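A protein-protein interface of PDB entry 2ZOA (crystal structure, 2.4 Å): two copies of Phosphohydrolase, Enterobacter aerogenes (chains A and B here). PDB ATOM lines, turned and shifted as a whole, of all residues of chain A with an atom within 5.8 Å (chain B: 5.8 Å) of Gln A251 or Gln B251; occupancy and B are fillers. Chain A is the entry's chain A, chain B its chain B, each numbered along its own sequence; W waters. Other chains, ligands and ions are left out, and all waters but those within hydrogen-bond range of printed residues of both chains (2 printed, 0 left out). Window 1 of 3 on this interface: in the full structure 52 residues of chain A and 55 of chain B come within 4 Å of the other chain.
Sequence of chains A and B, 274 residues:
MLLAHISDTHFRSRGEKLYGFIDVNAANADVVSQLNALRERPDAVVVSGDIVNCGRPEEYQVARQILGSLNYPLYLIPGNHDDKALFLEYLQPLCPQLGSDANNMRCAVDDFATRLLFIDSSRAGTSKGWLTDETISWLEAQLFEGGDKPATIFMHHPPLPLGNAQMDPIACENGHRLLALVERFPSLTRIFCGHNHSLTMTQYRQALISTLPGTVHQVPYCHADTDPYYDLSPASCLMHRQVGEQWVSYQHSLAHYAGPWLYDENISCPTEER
N of Gln B251 sits at hydrogen-bond distance from O of Leu A199. The backbone carbonyl oxygen (O) of Leu B199 is in hydrogen-bond range of the backbone NH (N) of Gln A251. The side-chain amide nitrogen (NE2) of Gln A251 sits at hydrogen-bond distance from the side-chain amide oxygen (OE1) of Gln B251, 2.8 Å away.
The side-chain amide nitrogen (NE2) of Gln A251 is in hydrogen-bond range of the side-chain hydroxyl (OG) of Ser A236 (3.0 Å). The backbone NH of Met A239 sits at hydrogen-bond distance from the backbone carbonyl oxygen of Tyr A250 (2.8 Å). OG of Ser B236 sits at hydrogen-bond distance from NE2 of Gln B251 (2.8 Å). N of Met B239 lies within hydrogen-bond range of O of Tyr B250.
O of Leu A199 touches O of Ser B249, 3.98 Å away. CA of Tyr B250 touches O of Leu A199, at 3.3 Å. CA of Thr A200 touches O of Ser B249, at 3.1 Å. CB of Thr A200 touches CB of Tyr B250, 3.6 Å away. O of Ser A249 touches O of Leu B199, 3.9 Å away. Thr B200 touches Ser A249 (CA to O, 3.1 Å). Tyr A250 touches Leu B199. CB of Thr B200 touches CB of Tyr A250 (3.6 Å).
Printed residues of chain B within 4 Å of Ser A249: Leu B199 (3.9 Å) and Thr B200 (3.1 Å). Printed residues of chain B within 4 Å of Tyr A250: Leu B199 and Thr B200. Of the printed residues of chain A, Leu B199 touches Ser A249, Tyr A250 and Gln A251. Printed residues of chain A within 4 Å of Thr B200: Ser A249 (3.1 Å) and Tyr A250 (3.6 Å). Cys B237 touches none of the printed residues of chain A. Met B239 touches none of the printed residues of chain A. Of the printed residues of chain A, Ser B249 touches Leu A199 and Thr A200. Of chain A, only Leu A199 (2.9 Å) and Gln A251 (2.8 Å) come within 4 Å of Gln B251. The nearest residue of chain A that does not touch Gln B251 is Pro A213 (4.8 Å). The nearest printed residue of chain B that does not touch Tyr A250 is Ser B198 (4.6 Å).
Printed residues of chain B that touch a printed residue of chain A: Leu B199, Thr B200, Ser B249, Tyr B250 and Gln B251. Of the 13 printed residues of chain A, 5 touch a printed residue of chain B. Hydrophobic or aromatic side chains of chain A within 4 Å of the printed part of chain B: Tyr A250. Among the printed residues, 11 pairs touch across the chains.
Leu A199 touches Ser B249, and with the chains exchanged Ser A249 touches Leu B199. Leu A199 touches Tyr B250, and with the chains exchanged Tyr A250 touches Leu B199. Leu A199 touches Gln B251, and with the chains exchanged Gln A251 touches Leu B199. Thr A200 touches Tyr B250, and with the chains exchanged Tyr A250 touches Thr B200. Positions printed for both chains: 198, 199, 200, 213, 236, 237, 238, 239, 249, 250, 251, 252 and 253. Of the 11 pairs that touch across the chains among the printed residues, 11 have their exchanged pair printed and touching as well.
Water W1 lies within hydrogen-bond range of the backbone NH of Leu B199 (2.8 Å) and the side-chain amide oxygen of Gln A251 (3.1 Å). Water W2 bridges the backbone NH of Leu A199 (2.8 Å) and the side-chain amide oxygen of Gln B251 (3.2 Å).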
ATOM      1  N   SER A 198      -8.549 -13.809  -6.017  1.00  0.00           N
ATOM      2  CA  SER A 198      -8.420 -14.583  -4.807  1.00  0.00           C
ATOM      3  C   SER A 198      -9.756 -14.484  -4.141  1.00  0.00           C
ATOM      4  O   SER A 198     -10.345 -13.395  -4.135  1.00  0.00           O
ATOM      5  CB  SER A 198      -7.409 -13.906  -3.893  1.00  0.00           C
ATOM      6  OG  SER A 198      -7.440 -14.504  -2.622  1.00  0.00           O
ATOM      7  N   LEU A 199     -10.243 -15.587  -3.583  1.00  0.00           N
ATOM      8  CA  LEU A 199     -11.364 -15.496  -2.669  1.00  0.00           C
ATOM      9  C   LEU A 199     -10.908 -15.025  -1.299  1.00  0.00           C
ATOM     10  O   LEU A 199     -10.302 -15.763  -0.530  1.00  0.00           O
ATOM     11  CB  LEU A 199     -12.148 -16.800  -2.566  1.00  0.00           C
ATOM     12  CG  LEU A 199     -13.563 -16.466  -2.101  1.00  0.00           C
ATOM     13  CD1 LEU A 199     -14.553 -17.288  -2.855  1.00  0.00           C
ATOM     14  CD2 LEU A 199     -13.702 -16.688  -0.608  1.00  0.00           C
ATOM     15  N   THR A 200     -11.178 -13.770  -0.997  1.00  0.00           N
ATOM     16  CA  THR A 200     -10.879 -13.294   0.333  1.00  0.00           C
ATOM     17  C   THR A 200     -12.085 -12.544   0.857  1.00  0.00           C
ATOM     18  O   THR A 200     -12.662 -11.730   0.142  1.00  0.00           O
ATOM     19  CB  THR A 200      -9.456 -12.562   0.490  1.00  0.00           C
ATOM     20  OG1 THR A 200      -9.588 -11.215   0.931  1.00  0.00           O
ATOM     21  CG2 THR A 200      -8.599 -12.611  -0.728  1.00  0.00           C
ATOM     22  N   PRO A 213     -12.019 -15.005  -7.044  1.00  0.00           N
ATOM     23  CA  PRO A 213     -10.999 -15.557  -7.930  1.00  0.00           C
ATOM     24  C   PRO A 213     -11.180 -15.024  -9.365  1.00  0.00           C
ATOM     25  O   PRO A 213     -12.298 -14.621  -9.750  1.00  0.00           O
ATOM     26  CB  PRO A 213     -11.316 -17.052  -7.912  1.00  0.00           C
ATOM     27  CG  PRO A 213     -12.021 -17.280  -6.637  1.00  0.00           C
ATOM     28  CD  PRO A 213     -12.872 -16.068  -6.476  1.00  0.00           C
ATOM     29  N   SER A 236     -12.405 -20.458 -10.423  1.00  0.00           N
ATOM     30  CA  SER A 236     -13.734 -20.737  -9.955  1.00  0.00           C
ATOM     31  C   SER A 236     -14.536 -19.491 -10.058  1.00  0.00           C
ATOM     32  O   SER A 236     -14.020 -18.408 -10.358  1.00  0.00           O
ATOM     33  CB  SER A 236     -13.740 -21.272  -8.521  1.00  0.00           C
ATOM     34  OG  SER A 236     -13.223 -20.326  -7.617  1.00  0.00           O
ATOM     35  N   CYS A 237     -15.826 -19.639  -9.858  1.00  0.00           N
ATOM     36  CA  CYS A 237     -16.605 -18.444  -9.743  1.00  0.00           C
ATOM     37  C   CYS A 237     -17.501 -18.553  -8.517  1.00  0.00           C
ATOM     38  O   CYS A 237     -17.475 -19.570  -7.811  1.00  0.00           O
ATOM     39  CB  CYS A 237     -17.399 -18.213 -11.015  1.00  0.00           C
ATOM     40  SG  CYS A 237     -18.682 -19.422 -11.280  1.00  0.00           S
ATOM     41  N   LEU A 238     -18.269 -17.491  -8.289  1.00  0.00           N
ATOM     42  CA  LEU A 238     -19.201 -17.408  -7.204  1.00  0.00           C
ATOM     43  C   LEU A 238     -20.622 -17.460  -7.772  1.00  0.00           C
ATOM     44  O   LEU A 238     -20.954 -16.739  -8.717  1.00  0.00           O
ATOM     45  CB  LEU A 238     -18.954 -16.097  -6.478  1.00  0.00           C
ATOM     46  CG  LEU A 238     -18.810 -16.125  -4.970  1.00  0.00           C
ATOM     47  CD1 LEU A 238     -17.992 -17.305  -4.508  1.00  0.00           C
ATOM     48  CD2 LEU A 238     -18.241 -14.797  -4.440  1.00  0.00           C
ATOM     49  N   MET A 239     -21.433 -18.373  -7.249  1.00  0.00           N
ATOM     50  CA  MET A 239     -22.867 -18.337  -7.492  1.00  0.00           C
ATOM     51  C   MET A 239     -23.541 -17.649  -6.305  1.00  0.00           C
ATOM     52  O   MET A 239     -23.275 -17.983  -5.146  1.00  0.00           O
ATOM     53  CB  MET A 239     -23.441 -19.736  -7.662  1.00  0.00           C
ATOM     54  CG  MET A 239     -22.763 -20.589  -8.694  1.00  0.00           C
ATOM     55  SD  MET A 239     -23.020 -20.102 -10.423  1.00  0.00           S
ATOM     56  CE  MET A 239     -24.784 -19.988 -10.525  1.00  0.00           C
ATOM     57  N   SER A 249     -23.703 -17.170  -1.051  1.00  0.00           N
ATOM     58  CA  SER A 249     -22.699 -17.268  -2.109  1.00  0.00           C
ATOM     59  C   SER A 249     -21.922 -18.564  -1.976  1.00  0.00           C
ATOM     60  O   SER A 249     -21.430 -18.911  -0.895  1.00  0.00           O
ATOM     61  CB  SER A 249     -21.723 -16.123  -2.007  1.00  0.00           C
ATOM     62  OG  SER A 249     -22.423 -14.932  -2.188  1.00  0.00           O
ATOM     63  N   TYR A 250     -21.822 -19.294  -3.072  1.00  0.00           N
ATOM     64  CA  TYR A 250     -21.045 -20.524  -3.062  1.00  0.00           C
ATOM     65  C   TYR A 250     -20.071 -20.576  -4.214  1.00  0.00           C
ATOM     66  O   TYR A 250     -20.325 -20.030  -5.301  1.00  0.00           O
ATOM     67  CB  TYR A 250     -21.919 -21.786  -3.011  1.00  0.00           C
ATOM     68  CG  TYR A 250     -22.928 -21.954  -4.107  1.00  0.00           C
ATOM     69  CD1 TYR A 250     -22.629 -22.719  -5.244  1.00  0.00           C
ATOM     70  CD2 TYR A 250     -24.205 -21.391  -3.999  1.00  0.00           C
ATOM     71  CE1 TYR A 250     -23.560 -22.906  -6.255  1.00  0.00           C
ATOM     72  CE2 TYR A 250     -25.150 -21.556  -5.016  1.00  0.00           C
ATOM     73  CZ  TYR A 250     -24.821 -22.324  -6.140  1.00  0.00           C
ATOM     74  OH  TYR A 250     -25.758 -22.518  -7.152  1.00  0.00           O
ATOM     75  N   GLN A 251     -18.947 -21.233  -3.950  1.00  0.00           N
ATOM     76  CA  GLN A 251     -17.895 -21.324  -4.934  1.00  0.00           C
ATOM     77  C   GLN A 251     -18.234 -22.454  -5.911  1.00  0.00           C
ATOM     78  O   GLN A 251     -18.595 -23.545  -5.505  1.00  0.00           O
ATOM     79  CB  GLN A 251     -16.569 -21.537  -4.251  1.00  0.00           C
ATOM     80  CG  GLN A 251     -15.424 -21.609  -5.191  1.00  0.00           C
ATOM     81  CD  GLN A 251     -14.140 -21.701  -4.437  1.00  0.00           C
ATOM     82  OE1 GLN A 251     -13.917 -22.667  -3.687  1.00  0.00           O
ATOM     83  NE2 GLN A 251     -13.276 -20.714  -4.620  1.00  0.00           N
ATOM     84  N   HIS A 252     -18.181 -22.141  -7.200  1.00  0.00           N
ATOM     85  CA  HIS A 252     -18.419 -23.120  -8.232  1.00  0.00           C
ATOM     86  C   HIS A 252     -17.108 -23.303  -8.993  1.00  0.00           C
ATOM     87  O   HIS A 252     -16.610 -22.349  -9.587  1.00  0.00           O
ATOM     88  CB  HIS A 252     -19.523 -22.628  -9.152  1.00  0.00           C
ATOM     89  CG  HIS A 252     -19.856 -23.588 -10.249  1.00  0.00           C
ATOM     90  ND1 HIS A 252     -19.295 -23.504 -11.505  1.00  0.00           N
ATOM     91  CD2 HIS A 252     -20.663 -24.672 -10.269  1.00  0.00           C
ATOM     92  CE1 HIS A 252     -19.741 -24.498 -12.252  1.00  0.00           C
ATOM     93  NE2 HIS A 252     -20.582 -25.214 -11.527  1.00  0.00           N
ATOM     94  N   SER A 253     -16.527 -24.506  -8.939  1.00  0.00           N
ATOM     95  CA  SER A 253     -15.259 -24.769  -9.595  1.00  0.00           C
ATOM     96  C   SER A 253     -15.386 -24.695 -11.116  1.00  0.00           C
ATOM     97  O   SER A 253     -16.319 -25.251 -11.715  1.00  0.00           O
ATOM     98  CB  SER A 253     -14.720 -26.131  -9.186  1.00  0.00           C
ATOM     99  OG  SER A 253     -13.469 -26.383  -9.811  1.00  0.00           O
ATOM    100  N   SER B 198     -17.560 -27.436   0.841  1.00  0.00           N
ATOM    101  CA  SER B 198     -17.888 -26.404  -0.110  1.00  0.00           C
ATOM    102  C   SER B 198     -17.665 -25.076   0.573  1.00  0.00           C
ATOM    103  O   SER B 198     -18.034 -24.917   1.736  1.00  0.00           O
ATOM    104  CB  SER B 198     -19.370 -26.520  -0.451  1.00  0.00           C
ATOM    105  OG  SER B 198     -19.768 -25.464  -1.284  1.00  0.00           O
ATOM    106  N   LEU B 199     -17.073 -24.122  -0.138  1.00  0.00           N
ATOM    107  CA  LEU B 199     -16.998 -22.756   0.341  1.00  0.00           C
ATOM    108  C   LEU B 199     -18.348 -22.064   0.051  1.00  0.00           C
ATOM    109  O   LEU B 199     -18.670 -21.687  -1.071  1.00  0.00           O
ATOM    110  CB  LEU B 199     -15.815 -22.017  -0.300  1.00  0.00           C
ATOM    111  CG  LEU B 199     -15.319 -20.714   0.328  1.00  0.00           C
ATOM    112  CD1 LEU B 199     -16.370 -19.588   0.206  1.00  0.00           C
ATOM    113  CD2 LEU B 199     -14.946 -20.933   1.803  1.00  0.00           C
ATOM    114  N   THR B 200     -19.166 -21.960   1.074  1.00  0.00           N
ATOM    115  CA  THR B 200     -20.429 -21.249   0.937  1.00  0.00           C
ATOM    116  C   THR B 200     -20.619 -20.254   2.094  1.00  0.00           C
ATOM    117  O   THR B 200     -20.491 -20.614   3.264  1.00  0.00           O
ATOM    118  CB  THR B 200     -21.674 -22.169   0.547  1.00  0.00           C
ATOM    119  OG1 THR B 200     -22.825 -21.853   1.340  1.00  0.00           O
ATOM    120  CG2 THR B 200     -21.392 -23.606   0.657  1.00  0.00           C
ATOM    121  N   PRO B 213     -14.390 -25.789   2.260  1.00  0.00           N
ATOM    122  CA  PRO B 213     -14.088 -26.993   1.476  1.00  0.00           C
ATOM    123  C   PRO B 213     -13.474 -28.109   2.344  1.00  0.00           C
ATOM    124  O   PRO B 213     -12.865 -27.825   3.401  1.00  0.00           O
ATOM    125  CB  PRO B 213     -13.049 -26.496   0.470  1.00  0.00           C
ATOM    126  CG  PRO B 213     -13.267 -25.053   0.384  1.00  0.00           C
ATOM    127  CD  PRO B 213     -13.646 -24.616   1.764  1.00  0.00           C
ATOM    128  N   SER B 236      -9.080 -27.030  -0.829  1.00  0.00           N
ATOM    129  CA  SER B 236      -8.456 -25.829  -0.321  1.00  0.00           C
ATOM    130  C   SER B 236      -8.643 -25.719   1.170  1.00  0.00           C
ATOM    131  O   SER B 236      -9.315 -26.554   1.800  1.00  0.00           O
ATOM    132  CB  SER B 236      -8.944 -24.565  -1.062  1.00  0.00           C
ATOM    133  OG  SER B 236     -10.317 -24.322  -0.868  1.00  0.00           O
ATOM    134  N   CYS B 237      -7.999 -24.722   1.755  1.00  0.00           N
ATOM    135  CA  CYS B 237      -8.348 -24.401   3.112  1.00  0.00           C
ATOM    136  C   CYS B 237      -8.527 -22.887   3.247  1.00  0.00           C
ATOM    137  O   CYS B 237      -8.370 -22.135   2.278  1.00  0.00           O
ATOM    138  CB  CYS B 237      -7.320 -24.959   4.067  1.00  0.00           C
ATOM    139  SG  CYS B 237      -5.770 -24.068   3.962  1.00  0.00           S
ATOM    140  N   LEU B 238      -8.911 -22.463   4.441  1.00  0.00           N
ATOM    141  CA  LEU B 238      -9.106 -21.064   4.713  1.00  0.00           C
ATOM    142  C   LEU B 238      -7.996 -20.620   5.639  1.00  0.00           C
ATOM    143  O   LEU B 238      -7.714 -21.269   6.626  1.00  0.00           O
ATOM    144  CB  LEU B 238     -10.486 -20.865   5.344  1.00  0.00           C
ATOM    145  CG  LEU B 238     -11.457 -19.859   4.733  1.00  0.00           C
ATOM    146  CD1 LEU B 238     -11.393 -19.835   3.229  1.00  0.00           C
ATOM    147  CD2 LEU B 238     -12.899 -20.084   5.208  1.00  0.00           C
ATOM    148  N   MET B 239      -7.336 -19.527   5.297  1.00  0.00           N
ATOM    149  CA  MET B 239      -6.432 -18.882   6.220  1.00  0.00           C
ATOM    150  C   MET B 239      -7.195 -17.742   6.847  1.00  0.00           C
ATOM    151  O   MET B 239      -7.854 -16.980   6.137  1.00  0.00           O
ATOM    152  CB  MET B 239      -5.218 -18.358   5.471  1.00  0.00           C
ATOM    153  CG  MET B 239      -4.470 -19.409   4.715  1.00  0.00           C
ATOM    154  SD  MET B 239      -3.662 -20.656   5.760  1.00  0.00           S
ATOM    155  CE  MET B 239      -2.371 -19.722   6.542  1.00  0.00           C
ATOM    156  N   SER B 249     -10.453 -13.654   5.849  1.00  0.00           N
ATOM    157  CA  SER B 249     -10.333 -15.069   5.528  1.00  0.00           C
ATOM    158  C   SER B 249      -9.989 -15.136   4.059  1.00  0.00           C
ATOM    159  O   SER B 249     -10.603 -14.460   3.223  1.00  0.00           O
ATOM    160  CB  SER B 249     -11.638 -15.824   5.789  1.00  0.00           C
ATOM    161  OG  SER B 249     -11.951 -15.849   7.164  1.00  0.00           O
ATOM    162  N   TYR B 250      -8.960 -15.898   3.743  1.00  0.00           N
ATOM    163  CA  TYR B 250      -8.635 -16.088   2.347  1.00  0.00           C
ATOM    164  C   TYR B 250      -8.442 -17.549   2.016  1.00  0.00           C
ATOM    165  O   TYR B 250      -8.048 -18.338   2.866  1.00  0.00           O
ATOM    166  CB  TYR B 250      -7.452 -15.224   1.900  1.00  0.00           C
ATOM    167  CG  TYR B 250      -6.158 -15.440   2.621  1.00  0.00           C
ATOM    168  CD1 TYR B 250      -5.197 -16.325   2.107  1.00  0.00           C
ATOM    169  CD2 TYR B 250      -5.867 -14.735   3.795  1.00  0.00           C
ATOM    170  CE1 TYR B 250      -3.970 -16.502   2.729  1.00  0.00           C
ATOM    171  CE2 TYR B 250      -4.650 -14.918   4.460  1.00  0.00           C
ATOM    172  CZ  TYR B 250      -3.707 -15.799   3.915  1.00  0.00           C
ATOM    173  OH  TYR B 250      -2.500 -15.993   4.557  1.00  0.00           O
ATOM    174  N   GLN B 251      -8.774 -17.905   0.784  1.00  0.00           N
ATOM    175  CA  GLN B 251      -8.687 -19.277   0.346  1.00  0.00           C
ATOM    176  C   GLN B 251      -7.239 -19.619  -0.054  1.00  0.00           C
ATOM    177  O   GLN B 251      -6.605 -18.904  -0.798  1.00  0.00           O
ATOM    178  CB  GLN B 251      -9.672 -19.524  -0.789  1.00  0.00           C
ATOM    179  CG  GLN B 251      -9.690 -20.970  -1.279  1.00  0.00           C
ATOM    180  CD  GLN B 251     -10.791 -21.202  -2.301  1.00  0.00           C
ATOM    181  OE1 GLN B 251     -10.823 -20.562  -3.369  1.00  0.00           O
ATOM    182  NE2 GLN B 251     -11.687 -22.118  -1.989  1.00  0.00           N
ATOM    183  N   HIS B 252      -6.704 -20.698   0.498  1.00  0.00           N
ATOM    184  CA  HIS B 252      -5.363 -21.154   0.137  1.00  0.00           C
ATOM    185  C   HIS B 252      -5.507 -22.500  -0.566  1.00  0.00           C
ATOM    186  O   HIS B 252      -5.999 -23.455   0.017  1.00  0.00           O
ATOM    187  CB  HIS B 252      -4.515 -21.272   1.395  1.00  0.00           C
ATOM    188  CG  HIS B 252      -3.122 -21.719   1.123  1.00  0.00           C
ATOM    189  ND1 HIS B 252      -2.741 -23.041   1.202  1.00  0.00           N
ATOM    190  CD2 HIS B 252      -2.029 -21.031   0.733  1.00  0.00           C
ATOM    191  CE1 HIS B 252      -1.467 -23.149   0.866  1.00  0.00           C
ATOM    192  NE2 HIS B 252      -1.014 -21.944   0.581  1.00  0.00           N
ATOM    193  N   SER B 253      -5.117 -22.559  -1.840  1.00  0.00           N
ATOM    194  CA  SER B 253      -5.256 -23.770  -2.649  1.00  0.00           C
ATOM    195  C   SER B 253      -4.368 -24.888  -2.117  1.00  0.00           C
ATOM    196  O   SER B 253      -3.175 -24.666  -1.846  1.00  0.00           O
ATOM    197  CB  SER B 253      -4.868 -23.490  -4.095  1.00  0.00           C
ATOM    198  OG  SER B 253      -5.147 -24.637  -4.863  1.00  0.00           O
HETATM  199  O   HOH W   1     -16.045 -24.707  -2.629  1.00  0.00           O
HETATM  200  O   HOH W   2      -8.960 -18.006  -3.964  1.00  0.00           O
